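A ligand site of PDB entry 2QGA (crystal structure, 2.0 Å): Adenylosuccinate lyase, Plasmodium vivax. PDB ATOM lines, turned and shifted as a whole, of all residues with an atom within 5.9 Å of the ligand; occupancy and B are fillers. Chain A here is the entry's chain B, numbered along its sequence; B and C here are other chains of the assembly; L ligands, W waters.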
ATOM      1  N   GLU A  83      -1.513  -7.810 -14.595  1.00  0.00           N
ATOM      2  CA  GLU A  83      -2.957  -7.902 -14.831  1.00  0.00           C
ATOM      3  C   GLU A  83      -3.365  -7.669 -16.284  1.00  0.00           C
ATOM      4  O   GLU A  83      -4.335  -8.254 -16.752  1.00  0.00           O
ATOM      5  CB  GLU A  83      -3.735  -6.966 -13.897  1.00  0.00           C
ATOM      6  CG  GLU A  83      -5.229  -7.318 -13.827  1.00  0.00           C
ATOM      7  CD  GLU A  83      -6.105  -6.282 -13.101  1.00  0.00           C
ATOM      8  OE1 GLU A  83      -5.584  -5.303 -12.532  1.00  0.00           O
ATOM      9  OE2 GLU A  83      -7.351  -6.461 -13.106  1.00  0.00           O
ATOM     10  N   THR A  86      -2.889 -11.191 -17.475  1.00  0.00           N
ATOM     11  CA  THR A  86      -3.786 -12.194 -16.900  1.00  0.00           C
ATOM     12  C   THR A  86      -5.266 -11.899 -17.085  1.00  0.00           C
ATOM     13  O   THR A  86      -6.080 -12.833 -17.202  1.00  0.00           O
ATOM     14  CB  THR A  86      -3.465 -12.452 -15.389  1.00  0.00           C
ATOM     15  OG1 THR A  86      -3.743 -11.275 -14.601  1.00  0.00           O
ATOM     16  CG2 THR A  86      -2.013 -12.861 -15.215  1.00  0.00           C
ATOM     17  N   ASN A  87      -5.637 -10.612 -17.110  1.00  0.00           N
ATOM     18  CA  ASN A  87      -7.018 -10.182 -16.892  1.00  0.00           C
ATOM     19  C   ASN A  87      -7.655 -10.896 -15.665  1.00  0.00           C
ATOM     20  O   ASN A  87      -8.830 -11.283 -15.677  1.00  0.00           O
ATOM     21  CB  ASN A  87      -7.863 -10.373 -18.168  1.00  0.00           C
ATOM     22  CG  ASN A  87      -9.241  -9.682 -18.089  1.00  0.00           C
ATOM     23  OD1 ASN A  87     -10.239 -10.208 -18.625  1.00  0.00           O
ATOM     24  ND2 ASN A  87      -9.304  -8.516 -17.412  1.00  0.00           N
ATOM     25  N   HIS A  88      -6.838 -11.074 -14.626  1.00  0.00           N
ATOM     26  CA  HIS A  88      -7.255 -11.682 -13.374  1.00  0.00           C
ATOM     27  C   HIS A  88      -6.422 -11.005 -12.292  1.00  0.00           C
ATOM     28  O   HIS A  88      -5.180 -11.168 -12.259  1.00  0.00           O
ATOM     29  CB  HIS A  88      -7.048 -13.208 -13.380  1.00  0.00           C
ATOM     30  CG  HIS A  88      -7.804 -13.942 -12.308  1.00  0.00           C
ATOM     31  ND1 HIS A  88      -7.621 -13.710 -10.963  1.00  0.00           N
ATOM     32  CD2 HIS A  88      -8.754 -14.900 -12.393  1.00  0.00           C
ATOM     33  CE1 HIS A  88      -8.419 -14.501 -10.263  1.00  0.00           C
ATOM     34  NE2 HIS A  88      -9.105 -15.237 -11.107  1.00  0.00           N
ATOM     35  N   ASP A  89      -7.094 -10.236 -11.430  1.00  0.00           N
ATOM     36  CA  ASP A  89      -6.408  -9.347 -10.503  1.00  0.00           C
ATOM     37  C   ASP A  89      -5.658 -10.094  -9.398  1.00  0.00           C
ATOM     38  O   ASP A  89      -4.480  -9.803  -9.162  1.00  0.00           O
ATOM     39  CB  ASP A  89      -7.322  -8.184  -9.964  1.00  0.00           C
ATOM     40  CG  ASP A  89      -8.699  -8.660  -9.348  1.00  0.00           C
ATOM     41  OD1 ASP A  89      -9.508  -7.769  -8.945  1.00  0.00           O
ATOM     42  OD2 ASP A  89      -8.965  -9.891  -9.224  1.00  0.00           O
ATOM     43  N   VAL A  90      -6.309 -11.071  -8.760  1.00  0.00           N
ATOM     44  CA  VAL A  90      -5.666 -11.842  -7.679  1.00  0.00           C
ATOM     45  C   VAL A  90      -4.532 -12.723  -8.206  1.00  0.00           C
ATOM     46  O   VAL A  90      -3.523 -12.880  -7.542  1.00  0.00           O
ATOM     47  CB  VAL A  90      -6.648 -12.702  -6.855  1.00  0.00           C
ATOM     48  CG1 VAL A  90      -5.875 -13.608  -5.878  1.00  0.00           C
ATOM     49  CG2 VAL A  90      -7.636 -11.780  -6.084  1.00  0.00           C
ATOM     50  N   THR A 121      -8.505 -20.082  -2.861  1.00  0.00           N
ATOM     51  CA  THR A 121      -9.214 -19.497  -3.989  1.00  0.00           C
ATOM     52  C   THR A 121      -9.032 -17.966  -3.905  1.00  0.00           C
ATOM     53  O   THR A 121      -8.648 -17.438  -2.865  1.00  0.00           O
ATOM     54  CB  THR A 121     -10.715 -19.943  -4.079  1.00  0.00           C
ATOM     55  OG1 THR A 121     -11.242 -19.551  -5.354  1.00  0.00           O
ATOM     56  CG2 THR A 121     -11.537 -19.329  -2.991  1.00  0.00           C
ATOM     57  N   SER A 122      -9.258 -17.242  -4.996  1.00  0.00           N
ATOM     58  CA  SER A 122      -9.020 -15.772  -4.947  1.00  0.00           C
ATOM     59  C   SER A 122      -9.828 -15.087  -3.836  1.00  0.00           C
ATOM     60  O   SER A 122      -9.327 -14.191  -3.200  1.00  0.00           O
ATOM     61  CB  SER A 122      -9.331 -15.115  -6.294  1.00  0.00           C
ATOM     62  OG  SER A 122      -8.509 -15.642  -7.303  1.00  0.00           O
ATOM     63  N   GLU A 123     -11.067 -15.551  -3.601  1.00  0.00           N
ATOM     64  CA  GLU A 123     -11.959 -14.948  -2.593  1.00  0.00           C
ATOM     65  C   GLU A 123     -11.476 -15.165  -1.163  1.00  0.00           C
ATOM     66  O   GLU A 123     -11.890 -14.423  -0.264  1.00  0.00           O
ATOM     67  CB  GLU A 123     -13.389 -15.518  -2.748  1.00  0.00           C
ATOM     68  CG  GLU A 123     -14.112 -15.000  -3.977  1.00  0.00           C
ATOM     69  CD  GLU A 123     -14.226 -13.490  -4.014  1.00  0.00           C
ATOM     70  OE1 GLU A 123     -14.317 -12.845  -2.925  1.00  0.00           O
ATOM     71  OE2 GLU A 123     -14.205 -12.959  -5.129  1.00  0.00           O
ATOM     72  N   ASN A 126      -9.422 -12.056  -1.136  1.00  0.00           N
ATOM     73  CA  ASN A 126     -10.285 -10.859  -1.254  1.00  0.00           C
ATOM     74  C   ASN A 126     -11.063 -10.602   0.031  1.00  0.00           C
ATOM     75  O   ASN A 126     -11.087  -9.481   0.538  1.00  0.00           O
ATOM     76  CB  ASN A 126     -11.309 -11.025  -2.382  1.00  0.00           C
ATOM     77  CG  ASN A 126     -10.700 -10.869  -3.760  1.00  0.00           C
ATOM     78  OD1 ASN A 126      -9.652 -10.239  -3.912  1.00  0.00           O
ATOM     79  ND2 ASN A 126     -11.353 -11.429  -4.788  1.00  0.00           N
ATOM     80  N   GLN A 247     -17.814 -20.435  -2.590  1.00  0.00           N
ATOM     81  CA  GLN A 247     -16.613 -19.721  -3.009  1.00  0.00           C
ATOM     82  C   GLN A 247     -16.513 -18.335  -2.333  1.00  0.00           C
ATOM     83  O   GLN A 247     -15.423 -17.856  -2.011  1.00  0.00           O
ATOM     84  CB  GLN A 247     -16.554 -19.608  -4.509  1.00  0.00           C
ATOM     85  CG  GLN A 247     -15.359 -18.764  -4.988  1.00  0.00           C
ATOM     86  CD  GLN A 247     -15.092 -18.905  -6.451  1.00  0.00           C
ATOM     87  OE1 GLN A 247     -15.406 -18.000  -7.254  1.00  0.00           O
ATOM     88  NE2 GLN A 247     -14.512 -20.061  -6.835  1.00  0.00           N
ATOM     89  N   ARG A 335     -21.241 -19.312  -6.639  1.00  0.00           N
ATOM     90  CA  ARG A 335     -21.248 -17.825  -6.670  1.00  0.00           C
ATOM     91  C   ARG A 335     -21.342 -17.344  -8.137  1.00  0.00           C
ATOM     92  O   ARG A 335     -20.989 -18.075  -9.088  1.00  0.00           O
ATOM     93  CB  ARG A 335     -20.036 -17.170  -5.973  1.00  0.00           C
ATOM     94  CG  ARG A 335     -18.626 -17.415  -6.678  1.00  0.00           C
ATOM     95  CD  ARG A 335     -18.288 -16.431  -7.808  1.00  0.00           C
ATOM     96  NE  ARG A 335     -18.215 -15.048  -7.328  1.00  0.00           N
ATOM     97  CZ  ARG A 335     -17.122 -14.475  -6.822  1.00  0.00           C
ATOM     98  NH1 ARG A 335     -16.001 -15.155  -6.739  1.00  0.00           N
ATOM     99  NH2 ARG A 335     -17.160 -13.198  -6.409  1.00  0.00           N
ATOM    100  N   LEU A 337     -20.125 -13.698 -10.281  1.00  0.00           N
ATOM    101  CA  LEU A 337     -19.127 -12.683 -10.011  1.00  0.00           C
ATOM    102  C   LEU A 337     -19.666 -11.264  -9.917  1.00  0.00           C
ATOM    103  O   LEU A 337     -18.863 -10.324  -9.748  1.00  0.00           O
ATOM    104  CB  LEU A 337     -17.988 -12.756 -11.034  1.00  0.00           C
ATOM    105  CG  LEU A 337     -16.647 -12.042 -10.776  1.00  0.00           C
ATOM    106  CD1 LEU A 337     -15.883 -12.579  -9.582  1.00  0.00           C
ATOM    107  CD2 LEU A 337     -15.818 -12.243 -12.037  1.00  0.00           C
ATOM    108  N   SER A 340     -18.388  -8.731  -7.137  1.00  0.00           N
ATOM    109  CA  SER A 340     -17.037  -8.205  -7.140  1.00  0.00           C
ATOM    110  C   SER A 340     -17.078  -6.715  -7.431  1.00  0.00           C
ATOM    111  O   SER A 340     -16.516  -5.900  -6.668  1.00  0.00           O
ATOM    112  CB  SER A 340     -16.168  -8.954  -8.185  1.00  0.00           C
ATOM    113  OG  SER A 340     -14.896  -8.321  -8.355  1.00  0.00           O
ATOM    114  N   THR A 341     -17.767  -6.340  -8.511  1.00  0.00           N
ATOM    115  CA  THR A 341     -17.764  -4.944  -8.891  1.00  0.00           C
ATOM    116  C   THR A 341     -18.554  -4.078  -7.887  1.00  0.00           C
ATOM    117  O   THR A 341     -18.180  -2.932  -7.618  1.00  0.00           O
ATOM    118  CB  THR A 341     -18.151  -4.728 -10.370  1.00  0.00           C
ATOM    119  OG1 THR A 341     -17.776  -3.390 -10.780  1.00  0.00           O
ATOM    120  CG2 THR A 341     -19.628  -4.954 -10.577  1.00  0.00           C
ATOM    121  N   ARG A 344     -16.505  -3.057  -4.801  1.00  0.00           N
ATOM    122  CA  ARG A 344     -15.520  -1.977  -5.095  1.00  0.00           C
ATOM    123  C   ARG A 344     -16.083  -0.592  -4.754  1.00  0.00           C
ATOM    124  O   ARG A 344     -15.354   0.377  -4.751  1.00  0.00           O
ATOM    125  CB  ARG A 344     -15.069  -2.014  -6.544  1.00  0.00           C
ATOM    126  CG  ARG A 344     -14.431  -3.330  -6.967  1.00  0.00           C
ATOM    127  CD  ARG A 344     -13.951  -3.234  -8.421  1.00  0.00           C
ATOM    128  NE  ARG A 344     -13.485  -4.546  -8.912  1.00  0.00           N
ATOM    129  CZ  ARG A 344     -12.273  -5.063  -8.629  1.00  0.00           C
ATOM    130  NH1 ARG A 344     -11.914  -6.246  -9.108  1.00  0.00           N
ATOM    131  NH2 ARG A 344     -11.415  -4.375  -7.861  1.00  0.00           N
ATOM    132  N   ARG B  14     -10.257   1.909 -10.970  1.00  0.00           N
ATOM    133  CA  ARG B  14     -10.179   0.703 -11.817  1.00  0.00           C
ATOM    134  C   ARG B  14     -10.785   0.862 -13.210  1.00  0.00           C
ATOM    135  O   ARG B  14     -10.203   0.383 -14.197  1.00  0.00           O
ATOM    136  CB  ARG B  14     -10.832  -0.506 -11.122  1.00  0.00           C
ATOM    137  CG  ARG B  14     -10.766  -1.797 -11.917  1.00  0.00           C
ATOM    138  CD  ARG B  14     -11.270  -2.971 -11.059  1.00  0.00           C
ATOM    139  NE  ARG B  14     -11.437  -4.215 -11.803  1.00  0.00           N
ATOM    140  CZ  ARG B  14     -10.432  -5.031 -12.150  1.00  0.00           C
ATOM    141  NH1 ARG B  14     -10.710  -6.128 -12.827  1.00  0.00           N
ATOM    142  NH2 ARG B  14      -9.155  -4.732 -11.858  1.00  0.00           N
ATOM    143  N   TYR B  15     -11.921   1.545 -13.309  1.00  0.00           N
ATOM    144  CA  TYR B  15     -12.637   1.661 -14.595  1.00  0.00           C
ATOM    145  C   TYR B  15     -12.451   2.980 -15.385  1.00  0.00           C
ATOM    146  O   TYR B  15     -13.202   3.254 -16.333  1.00  0.00           O
ATOM    147  CB  TYR B  15     -14.130   1.364 -14.402  1.00  0.00           C
ATOM    148  CG  TYR B  15     -14.429   0.099 -13.637  1.00  0.00           C
ATOM    149  CD1 TYR B  15     -14.024  -1.153 -14.116  1.00  0.00           C
ATOM    150  CD2 TYR B  15     -15.163   0.157 -12.458  1.00  0.00           C
ATOM    151  CE1 TYR B  15     -14.294  -2.312 -13.390  1.00  0.00           C
ATOM    152  CE2 TYR B  15     -15.471  -1.002 -11.752  1.00  0.00           C
ATOM    153  CZ  TYR B  15     -15.018  -2.227 -12.216  1.00  0.00           C
ATOM    154  OH  TYR B  15     -15.305  -3.340 -11.454  1.00  0.00           O
ATOM    155  N   GLY B 294      -8.530 -17.413 -17.514  1.00  0.00           N
ATOM    156  CA  GLY B 294      -9.955 -17.759 -17.424  1.00  0.00           C
ATOM    157  C   GLY B 294     -10.355 -18.131 -15.995  1.00  0.00           C
ATOM    158  O   GLY B 294     -10.891 -17.302 -15.242  1.00  0.00           O
ATOM    159  N   ASN B 303     -15.187 -18.115 -18.224  1.00  0.00           N
ATOM    160  CA  ASN B 303     -16.363 -17.650 -17.490  1.00  0.00           C
ATOM    161  C   ASN B 303     -16.974 -16.383 -18.103  1.00  0.00           C
ATOM    162  O   ASN B 303     -16.238 -15.575 -18.680  1.00  0.00           O
ATOM    163  CB  ASN B 303     -16.024 -17.423 -16.013  1.00  0.00           C
ATOM    164  CG  ASN B 303     -15.581 -18.709 -15.273  1.00  0.00           C
ATOM    165  OD1 ASN B 303     -14.522 -18.726 -14.643  1.00  0.00           O
ATOM    166  ND2 ASN B 303     -16.388 -19.773 -15.329  1.00  0.00           N
ATOM    167  N   ILE B 305     -17.495 -13.485 -17.356  1.00  0.00           N
ATOM    168  CA  ILE B 305     -17.198 -12.383 -16.422  1.00  0.00           C
ATOM    169  C   ILE B 305     -17.568 -10.992 -16.943  1.00  0.00           C
ATOM    170  O   ILE B 305     -17.738 -10.060 -16.111  1.00  0.00           O
ATOM    171  CB  ILE B 305     -15.749 -12.400 -15.887  1.00  0.00           C
ATOM    172  CG1 ILE B 305     -14.753 -12.042 -17.006  1.00  0.00           C
ATOM    173  CG2 ILE B 305     -15.419 -13.751 -15.255  1.00  0.00           C
ATOM    174  CD1 ILE B 305     -13.388 -11.629 -16.509  1.00  0.00           C
ATOM    175  N   GLU B 308     -21.227 -10.667 -16.012  1.00  0.00           N
ATOM    176  CA  GLU B 308     -21.344 -10.568 -14.533  1.00  0.00           C
ATOM    177  C   GLU B 308     -20.979  -9.157 -14.065  1.00  0.00           C
ATOM    178  O   GLU B 308     -21.623  -8.588 -13.200  1.00  0.00           O
ATOM    179  CB  GLU B 308     -20.499 -11.637 -13.842  1.00  0.00           C
ATOM    180  CG  GLU B 308     -21.007 -13.106 -14.140  1.00  0.00           C
ATOM    181  CD  GLU B 308     -20.092 -14.175 -13.557  1.00  0.00           C
ATOM    182  OE1 GLU B 308     -18.867 -14.192 -13.906  1.00  0.00           O
ATOM    183  OE2 GLU B 308     -20.589 -14.991 -12.734  1.00  0.00           O
ATOM    184  N   ASN B 309     -19.933  -8.595 -14.665  1.00  0.00           N
ATOM    185  CA  ASN B 309     -19.462  -7.262 -14.315  1.00  0.00           C
ATOM    186  C   ASN B 309     -20.526  -6.239 -14.732  1.00  0.00           C
ATOM    187  O   ASN B 309     -20.840  -5.312 -13.959  1.00  0.00           O
ATOM    188  CB  ASN B 309     -18.098  -6.978 -14.989  1.00  0.00           C
ATOM    189  CG  ASN B 309     -17.669  -5.519 -14.802  1.00  0.00           C
ATOM    190  OD1 ASN B 309     -16.894  -5.211 -13.898  1.00  0.00           O
ATOM    191  ND2 ASN B 309     -18.190  -4.603 -15.633  1.00  0.00           N
ATOM    192  N   THR C 169     -19.553 -22.220 -10.271  1.00  0.00           N
ATOM    193  CA  THR C 169     -19.106 -20.882  -9.966  1.00  0.00           C
ATOM    194  C   THR C 169     -19.131 -20.223 -11.344  1.00  0.00           C
ATOM    195  O   THR C 169     -18.679 -20.824 -12.329  1.00  0.00           O
ATOM    196  CB  THR C 169     -17.665 -20.886  -9.320  1.00  0.00           C
ATOM    197  OG1 THR C 169     -16.771 -21.572 -10.179  1.00  0.00           O
ATOM    198  CG2 THR C 169     -17.635 -21.596  -7.952  1.00  0.00           C
ATOM    199  N   HIS C 170     -19.678 -19.004 -11.429  1.00  0.00           N
ATOM    200  CA  HIS C 170     -20.055 -18.360 -12.710  1.00  0.00           C
ATOM    201  C   HIS C 170     -20.984 -19.215 -13.562  1.00  0.00           C
ATOM    202  O   HIS C 170     -20.964 -19.099 -14.782  1.00  0.00           O
ATOM    203  CB  HIS C 170     -18.860 -17.952 -13.578  1.00  0.00           C
ATOM    204  CG  HIS C 170     -17.660 -17.500 -12.818  1.00  0.00           C
ATOM    205  ND1 HIS C 170     -17.331 -16.177 -12.657  1.00  0.00           N
ATOM    206  CD2 HIS C 170     -16.680 -18.204 -12.209  1.00  0.00           C
ATOM    207  CE1 HIS C 170     -16.206 -16.084 -11.963  1.00  0.00           C
ATOM    208  NE2 HIS C 170     -15.793 -17.305 -11.678  1.00  0.00           N
HETATM  209  P1  LIG L   1     -14.573  -6.679 -11.679  1.00  0.00           P
HETATM  210  O1  LIG L   1     -14.763  -6.573 -10.179  1.00  0.00           O
HETATM  211  O2  LIG L   1     -15.743  -7.339 -12.394  1.00  0.00           O
HETATM  212  O3  LIG L   1     -14.016  -5.432 -12.357  1.00  0.00           O
HETATM  213  O4  LIG L   1     -13.344  -7.717 -11.836  1.00  0.00           O
HETATM  214  C1  LIG L   1     -13.454  -9.090 -11.462  1.00  0.00           C
HETATM  215  C2  LIG L   1     -12.050  -9.640 -11.370  1.00  0.00           C
HETATM  216  O5  LIG L   1     -12.096 -10.863 -10.666  1.00  0.00           O
HETATM  217  C3  LIG L   1     -11.447  -9.955 -12.736  1.00  0.00           C
HETATM  218  O6  LIG L   1     -10.038  -9.589 -12.687  1.00  0.00           O
HETATM  219  C4  LIG L   1     -11.668 -11.453 -12.883  1.00  0.00           C
HETATM  220  O7  LIG L   1     -10.737 -12.163 -13.720  1.00  0.00           O
HETATM  221  C5  LIG L   1     -11.469 -11.884 -11.449  1.00  0.00           C
HETATM  222  N1  LIG L   1     -12.031 -13.213 -11.168  1.00  0.00           N
HETATM  223  C6  LIG L   1     -12.412 -14.089 -12.117  1.00  0.00           C
HETATM  224  N2  LIG L   1     -12.907 -15.221 -11.555  1.00  0.00           N
HETATM  225  C7  LIG L   1     -12.838 -15.043 -10.221  1.00  0.00           C
HETATM  226  C8  LIG L   1     -13.185 -15.860  -9.067  1.00  0.00           C
HETATM  227  N3  LIG L   1     -13.729 -17.079  -9.287  1.00  0.00           N
HETATM  228  N4  LIG L   1     -12.982 -15.323  -7.827  1.00  0.00           N
HETATM  229  C9  LIG L   1     -12.480 -14.066  -7.634  1.00  0.00           C
HETATM  230  N5  LIG L   1     -12.115 -13.299  -8.653  1.00  0.00           N
HETATM  231  C10 LIG L   1     -12.273 -13.721  -9.946  1.00  0.00           C
HETATM  232  O   HOH W   1     -12.485 -17.130  -5.747  1.00  0.00           O
HETATM  233  O   HOH W   2     -18.090  -7.901 -10.998  1.00  0.00           O
HETATM  234  O   HOH W   3      -9.011  -8.059 -14.341  1.00  0.00           O
HETATM  235  O   HOH W   4     -13.256  -5.624 -14.822  1.00  0.00           O
HETATM  236  O   HOH W   5     -15.499  -9.280 -14.200  1.00  0.00           O
HETATM  237  O   HOH W   6     -10.952 -10.841  -7.629  1.00  0.00           O
HETATM  238  O   HOH W   7     -10.721 -17.714 -11.366  1.00  0.00           O
HETATM  239  O   HOH W   8     -11.008 -14.499 -15.869  1.00  0.00           O
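Water W3 lies within hydrogen-bond range of an oxygen (O6) of the ligand (2.5 Å), the side-chain carboxylate (OE2) of Glu 83 (2.6 Å), the guanidinium group (NH1) of Arg 14 of chain B (3.0 Å) and the side-chain amide nitrogen (ND2) of Asn 87 (3.1 Å). Water W4 bridges O3 of the ligand and NH1 of Arg 14 of chain B. Water W2 lies within hydrogen-bond range of an oxygen (O2) of the ligand (2.8 Å), the backbone carbonyl oxygen (O) of Leu 337 (2.8 Å) and the backbone NH (N) of Thr 341 (3.0 Å). Water W1 lies within hydrogen-bond range of the side-chain hydroxyl of Thr 121 (2.7 Å), a nitrogen (N4) of the ligand (2.8 Å), the backbone NH of Glu 123 (3.0 Å), the backbone NH of Ser 122 (3.3 Å) and the side-chain amide oxygen of Gln 247 (3.4 Å). Water W6 lies within hydrogen-bond range of OD2 of Asp 89 (2.7 Å), N5 of the ligand (2.9 Å) and ND2 of Asn 126 (2.9 Å). Water W8 bridges the backbone carbonyl oxygen (O) of Gly 294 of chain B (2.9 Å) and an oxygen (O7) of the ligand (3.2 Å).
Merely in contact with the ligand: Glu 123 (3.2 Å), His 88 (3.5 Å), Ser 122 (3.6 Å), Leu 337 (3.8 Å) and Ile 305 of chain B (3.9 Å). Of the 25 residues printed, 16 come within 4 Å of the ligand. Along chain A the residues within 4 Å of the ligand span positions 87 to 344.
The side-chain hydroxyl (OH) of Tyr 15 of chain B lies close to the guanidinium group (NE) of Arg 344 (3.4 Å). OH of Tyr 15 of chain B lies within hydrogen-bond range of OD1 of Asn 309 of chain B, at 3.5 Å. The side-chain hydroxyl (OG1) of Thr 341 sits at hydrogen-bond distance from the side-chain hydroxyl (OH) of Tyr 15 of chain B (2.6 Å). The guanidinium group of Arg 344 is in salt-bridge range of the side-chain carboxylate of Asp 89, at 2.9 Å. The side-chain amide oxygen (OE1) of Gln 247 is in hydrogen-bond range of the guanidinium group (NH1) of Arg 335 (3.0 Å). OE2 of Glu 123 sits at hydrogen-bond distance from ND2 of Asn 126, at 3.3 Å. The backbone carbonyl oxygen (O) of His 88 lies within hydrogen-bond range of the side-chain hydroxyl (OG1) of Thr 86, at 2.7 Å. The side-chain carboxylate of Glu 308 of chain B is in hydrogen-bond range of the backbone NH of Leu 337, at 2.8 Å.
The side-chain hydroxyl (OG) of Ser 340 lies within hydrogen-bond range of an oxygen (O1) of the ligand (2.5 Å). The side-chain hydroxyl of Tyr 15 of chain B sits at hydrogen-bond distance from an oxygen (O3) of the ligand. The guanidinium group (NE) of Arg 344 lies within salt-bridge range of an oxygen (O1) of the ligand (2.7 Å). A nitrogen (N3) of the ligand sits at hydrogen-bond distance from the side-chain amide oxygen (OE1) of Gln 247, 2.8 Å away. The side-chain amide oxygen (OD1) of Asn 309 of chain B sits close to an oxygen (O2) of the ligand. O7 of the ligand lies within hydrogen-bond range of O of Asn 87, 2.9 Å away. O3 of the ligand is in salt-bridge range of NE of Arg 14 of chain B (2.9 Å). A ring nitrogen (NE2) of His 170 of chain C lies within hydrogen-bond range of a nitrogen (N3) of the ligand, at 3.2 Å. A nitrogen (N4) of the ligand is in hydrogen-bond range of the guanidinium group (NH1) of Arg 335 (3.2 Å). An oxygen (O6) of the ligand sits at hydrogen-bond distance from the backbone NH of Asp 89, 3.3 Å away. O1 of the ligand is in hydrogen-bond range of N of Thr 341.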
